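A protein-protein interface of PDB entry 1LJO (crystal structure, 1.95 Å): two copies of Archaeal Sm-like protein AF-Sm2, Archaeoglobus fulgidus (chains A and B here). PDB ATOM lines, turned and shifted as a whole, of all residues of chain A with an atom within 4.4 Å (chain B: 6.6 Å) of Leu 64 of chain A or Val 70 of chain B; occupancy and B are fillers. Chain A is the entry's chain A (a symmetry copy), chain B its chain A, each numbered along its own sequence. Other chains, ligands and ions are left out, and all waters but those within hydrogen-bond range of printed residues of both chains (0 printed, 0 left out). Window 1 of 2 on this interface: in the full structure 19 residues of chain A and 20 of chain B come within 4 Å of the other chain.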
ATOM      1  N   VAL A  20      35.771   5.875  20.195  1.00  0.00           N
ATOM      2  CA  VAL A  20      35.052   5.211  21.281  1.00  0.00           C
ATOM      3  C   VAL A  20      33.734   4.572  20.872  1.00  0.00           C
ATOM      4  O   VAL A  20      32.928   5.189  20.183  1.00  0.00           O
ATOM      5  CB  VAL A  20      34.715   6.209  22.411  1.00  0.00           C
ATOM      6  CG1 VAL A  20      34.060   5.476  23.583  1.00  0.00           C
ATOM      7  CG2 VAL A  20      35.969   6.936  22.851  1.00  0.00           C
ATOM      8  N   MET A  22      30.262   3.185  22.299  1.00  0.00           N
ATOM      9  CA  MET A  22      29.412   3.251  23.484  1.00  0.00           C
ATOM     10  C   MET A  22      28.312   2.207  23.416  1.00  0.00           C
ATOM     11  O   MET A  22      27.810   1.886  22.337  1.00  0.00           O
ATOM     12  CB  MET A  22      28.763   4.635  23.612  1.00  0.00           C
ATOM     13  CG  MET A  22      29.728   5.797  23.736  1.00  0.00           C
ATOM     14  SD  MET A  22      30.735   5.727  25.234  1.00  0.00           S
ATOM     15  CE  MET A  22      29.515   6.128  26.493  1.00  0.00           C
ATOM     16  N   GLY A  24      25.186   2.437  24.523  1.00  0.00           N
ATOM     17  CA  GLY A  24      23.928   3.016  24.077  1.00  0.00           C
ATOM     18  C   GLY A  24      24.064   3.906  22.852  1.00  0.00           C
ATOM     19  O   GLY A  24      23.360   4.912  22.723  1.00  0.00           O
ATOM     20  N   ASN A  41      35.221   7.854  32.732  1.00  0.00           N
ATOM     21  CA  ASN A  41      34.308   8.829  32.151  1.00  0.00           C
ATOM     22  C   ASN A  41      35.261   9.528  31.188  1.00  0.00           C
ATOM     23  O   ASN A  41      36.449   9.641  31.482  1.00  0.00           O
ATOM     24  CB  ASN A  41      33.811   9.826  33.196  1.00  0.00           C
ATOM     25  CG  ASN A  41      32.845   9.202  34.177  1.00  0.00           C
ATOM     26  OD1 ASN A  41      31.923   8.491  33.778  1.00  0.00           O
ATOM     27  ND2 ASN A  41      33.049   9.464  35.467  1.00  0.00           N
ATOM     28  N   LEU A  42      34.765   9.978  30.042  1.00  0.00           N
ATOM     29  CA  LEU A  42      35.632  10.630  29.073  1.00  0.00           C
ATOM     30  C   LEU A  42      35.110  11.996  28.648  1.00  0.00           C
ATOM     31  O   LEU A  42      33.909  12.183  28.456  1.00  0.00           O
ATOM     32  CB  LEU A  42      35.777   9.756  27.819  1.00  0.00           C
ATOM     33  CG  LEU A  42      36.140   8.278  27.989  1.00  0.00           C
ATOM     34  CD1 LEU A  42      36.029   7.579  26.641  1.00  0.00           C
ATOM     35  CD2 LEU A  42      37.545   8.138  28.565  1.00  0.00           C
ATOM     36  N   LEU A  44      35.669  14.551  25.641  1.00  0.00           N
ATOM     37  CA  LEU A  44      36.234  14.753  24.314  1.00  0.00           C
ATOM     38  C   LEU A  44      35.883  16.138  23.797  1.00  0.00           C
ATOM     39  O   LEU A  44      34.824  16.676  24.116  1.00  0.00           O
ATOM     40  CB  LEU A  44      35.676  13.720  23.329  1.00  0.00           C
ATOM     41  CG  LEU A  44      35.849  12.232  23.638  1.00  0.00           C
ATOM     42  CD1 LEU A  44      35.306  11.407  22.477  1.00  0.00           C
ATOM     43  CD2 LEU A  44      37.317  11.927  23.863  1.00  0.00           C
ATOM     44  N   ILE A  62      31.845  16.907  24.300  1.00  0.00           N
ATOM     45  CA  ILE A  62      30.921  15.910  24.846  1.00  0.00           C
ATOM     46  C   ILE A  62      31.560  15.147  25.995  1.00  0.00           C
ATOM     47  O   ILE A  62      32.774  14.992  26.050  1.00  0.00           O
ATOM     48  CB  ILE A  62      30.477  14.860  23.797  1.00  0.00           C
ATOM     49  CG1 ILE A  62      31.704  14.148  23.222  1.00  0.00           C
ATOM     50  CG2 ILE A  62      29.658  15.519  22.689  1.00  0.00           C
ATOM     51  CD1 ILE A  62      31.359  12.985  22.306  1.00  0.00           C
ATOM     52  N   VAL A  63      30.724  14.667  26.907  1.00  0.00           N
ATOM     53  CA  VAL A  63      31.191  13.885  28.039  1.00  0.00           C
ATOM     54  C   VAL A  63      30.556  12.503  27.927  1.00  0.00           C
ATOM     55  O   VAL A  63      29.331  12.383  27.828  1.00  0.00           O
ATOM     56  CB  VAL A  63      30.779  14.531  29.377  1.00  0.00           C
ATOM     57  CG1 VAL A  63      31.052  13.576  30.526  1.00  0.00           C
ATOM     58  CG2 VAL A  63      31.536  15.845  29.570  1.00  0.00           C
ATOM     59  N   LEU A  64      31.388  11.466  27.927  1.00  0.00           N
ATOM     60  CA  LEU A  64      30.900  10.093  27.822  1.00  0.00           C
ATOM     61  C   LEU A  64      30.926   9.414  29.194  1.00  0.00           C
ATOM     62  O   LEU A  64      31.920   9.494  29.916  1.00  0.00           O
ATOM     63  CB  LEU A  64      31.757   9.308  26.823  1.00  0.00           C
ATOM     64  CG  LEU A  64      31.867   9.934  25.420  1.00  0.00           C
ATOM     65  CD1 LEU A  64      32.738   9.059  24.515  1.00  0.00           C
ATOM     66  CD2 LEU A  64      30.482  10.094  24.825  1.00  0.00           C
ATOM     67  N   ARG A  65      29.825   8.757  29.552  1.00  0.00           N
ATOM     68  CA  ARG A  65      29.728   8.073  30.838  1.00  0.00           C
ATOM     69  C   ARG A  65      30.551   6.787  30.809  1.00  0.00           C
ATOM     70  O   ARG A  65      30.329   5.921  29.971  1.00  0.00           O
ATOM     71  CB  ARG A  65      28.268   7.749  31.151  1.00  0.00           C
ATOM     72  CG  ARG A  65      28.036   7.146  32.518  1.00  0.00           C
ATOM     73  CD  ARG A  65      28.346   8.154  33.616  1.00  0.00           C
ATOM     74  NE  ARG A  65      28.032   7.625  34.939  1.00  0.00           N
ATOM     75  CZ  ARG A  65      28.858   6.888  35.671  1.00  0.00           C
ATOM     76  NH1 ARG A  65      30.066   6.586  35.211  1.00  0.00           N
ATOM     77  NH2 ARG A  65      28.475   6.456  36.867  1.00  0.00           N
ATOM     78  N   GLY A  66      31.491   6.675  31.743  1.00  0.00           N
ATOM     79  CA  GLY A  66      32.364   5.515  31.808  1.00  0.00           C
ATOM     80  C   GLY A  66      31.753   4.123  31.801  1.00  0.00           C
ATOM     81  O   GLY A  66      32.240   3.241  31.090  1.00  0.00           O
ATOM     82  N   ASN A  68      29.282   3.137  30.375  1.00  0.00           N
ATOM     83  CA  ASN A  68      28.640   2.842  29.095  1.00  0.00           C
ATOM     84  C   ASN A  68      29.638   2.838  27.943  1.00  0.00           C
ATOM     85  O   ASN A  68      29.274   2.686  26.765  1.00  0.00           O
ATOM     86  CB  ASN A  68      27.478   3.802  28.842  1.00  0.00           C
ATOM     87  CG  ASN A  68      26.289   3.484  29.734  1.00  0.00           C
ATOM     88  OD1 ASN A  68      25.936   2.318  29.899  1.00  0.00           O
ATOM     89  ND2 ASN A  68      25.679   4.504  30.315  1.00  0.00           N
ATOM     90  N   PRO B   6      36.198  14.938  33.623  1.00  0.00           N
ATOM     91  CA  PRO B   6      34.811  14.879  33.163  1.00  0.00           C
ATOM     92  C   PRO B   6      33.839  15.500  34.173  1.00  0.00           C
ATOM     93  O   PRO B   6      32.988  16.302  33.803  1.00  0.00           O
ATOM     94  CB  PRO B   6      34.589  13.387  32.959  1.00  0.00           C
ATOM     95  CG  PRO B   6      35.930  12.943  32.439  1.00  0.00           C
ATOM     96  CD  PRO B   6      36.880  13.649  33.396  1.00  0.00           C
ATOM     97  N   VAL B  20      21.127  15.329  26.480  1.00  0.00           N
ATOM     98  CA  VAL B  20      21.556  14.049  27.041  1.00  0.00           C
ATOM     99  C   VAL B  20      20.996  12.826  26.332  1.00  0.00           C
ATOM    100  O   VAL B  20      19.802  12.757  26.056  1.00  0.00           O
ATOM    101  CB  VAL B  20      21.130  13.924  28.521  1.00  0.00           C
ATOM    102  CG1 VAL B  20      21.680  12.627  29.118  1.00  0.00           C
ATOM    103  CG2 VAL B  20      21.604  15.132  29.300  1.00  0.00           C
ATOM    104  N   GLU B  21      21.864  11.861  26.047  1.00  0.00           N
ATOM    105  CA  GLU B  21      21.416  10.623  25.424  1.00  0.00           C
ATOM    106  C   GLU B  21      21.458   9.559  26.516  1.00  0.00           C
ATOM    107  O   GLU B  21      22.498   9.352  27.145  1.00  0.00           O
ATOM    108  CB  GLU B  21      22.333  10.226  24.267  1.00  0.00           C
ATOM    109  CG  GLU B  21      22.031   8.842  23.717  1.00  0.00           C
ATOM    110  CD  GLU B  21      22.797   8.539  22.448  1.00  0.00           C
ATOM    111  OE1 GLU B  21      24.030   8.734  22.435  1.00  0.00           O
ATOM    112  OE2 GLU B  21      22.161   8.101  21.464  1.00  0.00           O
ATOM    113  N   MET B  22      20.323   8.904  26.749  1.00  0.00           N
ATOM    114  CA  MET B  22      20.222   7.870  27.775  1.00  0.00           C
ATOM    115  C   MET B  22      20.205   6.488  27.147  1.00  0.00           C
ATOM    116  O   MET B  22      19.673   6.297  26.051  1.00  0.00           O
ATOM    117  CB  MET B  22      18.941   8.046  28.600  1.00  0.00           C
ATOM    118  CG  MET B  22      18.816   9.365  29.335  1.00  0.00           C
ATOM    119  SD  MET B  22      20.093   9.601  30.591  1.00  0.00           S
ATOM    120  CE  MET B  22      19.566   8.430  31.848  1.00  0.00           C
ATOM    121  N   LYS B  23      20.766   5.521  27.859  1.00  0.00           N
ATOM    122  CA  LYS B  23      20.822   4.150  27.374  1.00  0.00           C
ATOM    123  C   LYS B  23      19.425   3.557  27.186  1.00  0.00           C
ATOM    124  O   LYS B  23      19.152   2.903  26.178  1.00  0.00           O
ATOM    125  CB  LYS B  23      21.643   3.297  28.345  1.00  0.00           C
ATOM    126  CG  LYS B  23      21.883   1.875  27.888  1.00  0.00           C
ATOM    127  CD  LYS B  23      23.025   1.240  28.669  1.00  0.00           C
ATOM    128  CE  LYS B  23      22.769   1.265  30.169  1.00  0.00           C
ATOM    129  NZ  LYS B  23      23.938   0.766  30.944  1.00  0.00           N
ATOM    130  N   GLY B  24      18.538   3.792  28.149  1.00  0.00           N
ATOM    131  CA  GLY B  24      17.185   3.267  28.051  1.00  0.00           C
ATOM    132  C   GLY B  24      16.184   4.259  27.481  1.00  0.00           C
ATOM    133  O   GLY B  24      15.019   4.281  27.887  1.00  0.00           O
ATOM    134  N   MET B  40      27.258  11.257  38.295  1.00  0.00           N
ATOM    135  CA  MET B  40      26.658  11.848  37.106  1.00  0.00           C
ATOM    136  C   MET B  40      25.138  11.726  37.015  1.00  0.00           C
ATOM    137  O   MET B  40      24.569  11.675  35.917  1.00  0.00           O
ATOM    138  CB  MET B  40      27.327  11.308  35.835  1.00  0.00           C
ATOM    139  CG  MET B  40      28.671  11.991  35.568  1.00  0.00           C
ATOM    140  SD  MET B  40      29.453  11.583  33.994  1.00  0.00           S
ATOM    141  CE  MET B  40      28.192  12.014  32.892  1.00  0.00           C
ATOM    142  N   GLY B  66      22.538   8.462  36.637  1.00  0.00           N
ATOM    143  CA  GLY B  66      23.887   8.512  36.099  1.00  0.00           C
ATOM    144  C   GLY B  66      24.435   7.308  35.348  1.00  0.00           C
ATOM    145  O   GLY B  66      25.045   7.469  34.289  1.00  0.00           O
ATOM    146  N   ASN B  67      24.238   6.100  35.858  1.00  0.00           N
ATOM    147  CA  ASN B  67      24.800   4.961  35.144  1.00  0.00           C
ATOM    148  C   ASN B  67      24.076   4.654  33.840  1.00  0.00           C
ATOM    149  O   ASN B  67      24.510   3.793  33.087  1.00  0.00           O
ATOM    150  CB  ASN B  67      24.854   3.711  36.026  1.00  0.00           C
ATOM    151  CG  ASN B  67      23.497   3.241  36.449  1.00  0.00           C
ATOM    152  OD1 ASN B  67      22.852   3.855  37.295  1.00  0.00           O
ATOM    153  ND2 ASN B  67      23.045   2.139  35.857  1.00  0.00           N
ATOM    154  N   ASN B  68      22.978   5.352  33.570  1.00  0.00           N
ATOM    155  CA  ASN B  68      22.260   5.134  32.315  1.00  0.00           C
ATOM    156  C   ASN B  68      22.425   6.304  31.352  1.00  0.00           C
ATOM    157  O   ASN B  68      21.828   6.344  30.264  1.00  0.00           O
ATOM    158  CB  ASN B  68      20.789   4.818  32.583  1.00  0.00           C
ATOM    159  CG  ASN B  68      20.616   3.419  33.151  1.00  0.00           C
ATOM    160  OD1 ASN B  68      21.241   2.476  32.671  1.00  0.00           O
ATOM    161  ND2 ASN B  68      19.783   3.279  34.170  1.00  0.00           N
ATOM    162  N   VAL B  69      23.261   7.254  31.757  1.00  0.00           N
ATOM    163  CA  VAL B  69      23.576   8.400  30.911  1.00  0.00           C
ATOM    164  C   VAL B  69      24.632   7.886  29.941  1.00  0.00           C
ATOM    165  O   VAL B  69      25.568   7.198  30.351  1.00  0.00           O
ATOM    166  CB  VAL B  69      24.203   9.563  31.715  1.00  0.00           C
ATOM    167  CG1 VAL B  69      24.794  10.595  30.758  1.00  0.00           C
ATOM    168  CG2 VAL B  69      23.148  10.222  32.597  1.00  0.00           C
ATOM    169  N   VAL B  70      24.479   8.192  28.659  1.00  0.00           N
ATOM    170  CA  VAL B  70      25.458   7.755  27.669  1.00  0.00           C
ATOM    171  C   VAL B  70      26.367   8.908  27.264  1.00  0.00           C
ATOM    172  O   VAL B  70      27.596   8.813  27.346  1.00  0.00           O
ATOM    173  CB  VAL B  70      24.768   7.197  26.393  1.00  0.00           C
ATOM    174  CG1 VAL B  70      25.820   6.873  25.328  1.00  0.00           C
ATOM    175  CG2 VAL B  70      23.966   5.943  26.743  1.00  0.00           C
ATOM    176  N   LEU B  71      25.753  10.010  26.856  1.00  0.00           N
ATOM    177  CA  LEU B  71      26.495  11.172  26.395  1.00  0.00           C
ATOM    178  C   LEU B  71      25.826  12.474  26.829  1.00  0.00           C
ATOM    179  O   LEU B  71      24.601  12.575  26.839  1.00  0.00           O
ATOM    180  CB  LEU B  71      26.603  11.102  24.861  1.00  0.00           C
ATOM    181  CG  LEU B  71      27.292  12.200  24.041  1.00  0.00           C
ATOM    182  CD1 LEU B  71      27.528  11.687  22.613  1.00  0.00           C
ATOM    183  CD2 LEU B  71      26.433  13.452  24.013  1.00  0.00           C
ATOM    184  N   ILE B  72      26.642  13.461  27.193  1.00  0.00           N
ATOM    185  CA  ILE B  72      26.148  14.773  27.606  1.00  0.00           C
ATOM    186  C   ILE B  72      26.812  15.798  26.702  1.00  0.00           C
ATOM    187  O   ILE B  72      28.020  15.758  26.497  1.00  0.00           O
ATOM    188  CB  ILE B  72      26.523  15.109  29.068  1.00  0.00           C
ATOM    189  CG1 ILE B  72      25.933  14.065  30.016  1.00  0.00           C
ATOM    190  CG2 ILE B  72      26.006  16.511  29.428  1.00  0.00           C
ATOM    191  CD1 ILE B  72      26.297  14.298  31.485  1.00  0.00           C
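The side-chain amino group (NZ) of Lys 23 of chain B lies within hydrogen-bond range of the side-chain amide oxygen (OD1) of Asn 68 of chain A.
The guanidinium group (NE) of Arg 65 of chain A is in hydrogen-bond range of the backbone carbonyl oxygen (O) of Gly 66 of chain B (3.1 Å).
The backbone carbonyl oxygen (O) of Asn 67 of chain B lies within hydrogen-bond range of the side-chain amide nitrogen (ND2) of Asn 68 of chain A (3.1 Å).
The backbone carbonyl oxygen (O) of Val 69 of chain B is in hydrogen-bond range of the side-chain amide nitrogen (ND2) of Asn 68 of chain A.
The backbone carbonyl oxygen (O) of Val 70 of chain B lies within hydrogen-bond range of the backbone NH (N) of Arg 65 of chain A, at 3.1 Å.
O of Ile 72 of chain B sits at hydrogen-bond distance from N of Val 63 of chain A, 2.9 Å away.
The backbone NH (N) of Val 70 of chain B is in hydrogen-bond range of the backbone carbonyl oxygen (O) of Glu 21 of chain B (2.7 Å).
The backbone NH (N) of Glu 21 of chain B sits at hydrogen-bond distance from the backbone carbonyl oxygen (O) of Leu 71 of chain B (2.9 Å).
The backbone NH of Lys 23 of chain B is in hydrogen-bond range of the backbone carbonyl oxygen of Asn 68 of chain B (2.8 Å).
The side-chain amide oxygen of Asn 41 of chain A is in hydrogen-bond range of the backbone NH of Gly 66 of chain A (2.8 Å).
O of Leu 42 of chain A sits at hydrogen-bond distance from N of Leu 64 of chain A, at 2.7 Å.
N of Leu 44 of chain A is in hydrogen-bond range of O of Ile 62 of chain A, at 3.0 Å.
Among the printed residues, merely in contact across the chains: Arg 65 of chain A with Val 69 of chain B, Ile 62 of chain A with Ile 72 of chain B, Val 63 of chain A with Leu 71 of chain B, Met 22 of chain A with Val 70 of chain B, Asn 41 of chain A with Pro 6 of chain B, Leu 64 of chain A with Val 70 of chain B, Arg 65 of chain A with Met 40 of chain B, Gly 24 of chain A with Glu 21 of chain B, Asn 68 of chain A with Asn 68 of chain B, Leu 64 of chain A with Leu 71 of chain B, Gly 24 of chain A with Val 70 of chain B, Asn 41 of chain A with Met 40 of chain B, Leu 42 of chain A with Pro 6 of chain B and Val 63 of chain A with Val 70 of chain B.
Of the printed residues of chain B, Arg 65 of chain A touches Met 40, Gly 66, Val 69 and Val 70.
Of the printed residues of chain A, Asn 68 of chain B touches Asn 68 (3.9 Å).
Of the printed residues of chain A, Val 69 of chain B touches Arg 65 and Asn 68.
Of the printed residues of chain A, Val 70 of chain B touches Met 22, Gly 24, Val 63, Leu 64 and Arg 65.
Hydrophobic or aromatic side chains of chain B that line the printed part of chain A: Pro 6, Met 40, Val 70 and Leu 71.
Printed residues of chain A that touch a printed residue of chain B: Met 22, Gly 24, Asn 41, Leu 42, Ile 62, Val 63, Leu 64, Arg 65 and Asn 68.
Among the printed residues, 20 pairs touch across the chains.
Asn 68 of chain A touches its own counterpart, Asn 68 of chain B.
Positions printed for both chains: 20, 22, 24, 66 and 68.
Of the 20 pairs that touch across the chains among the printed residues, 1 has its exchanged pair printed and touching as well.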
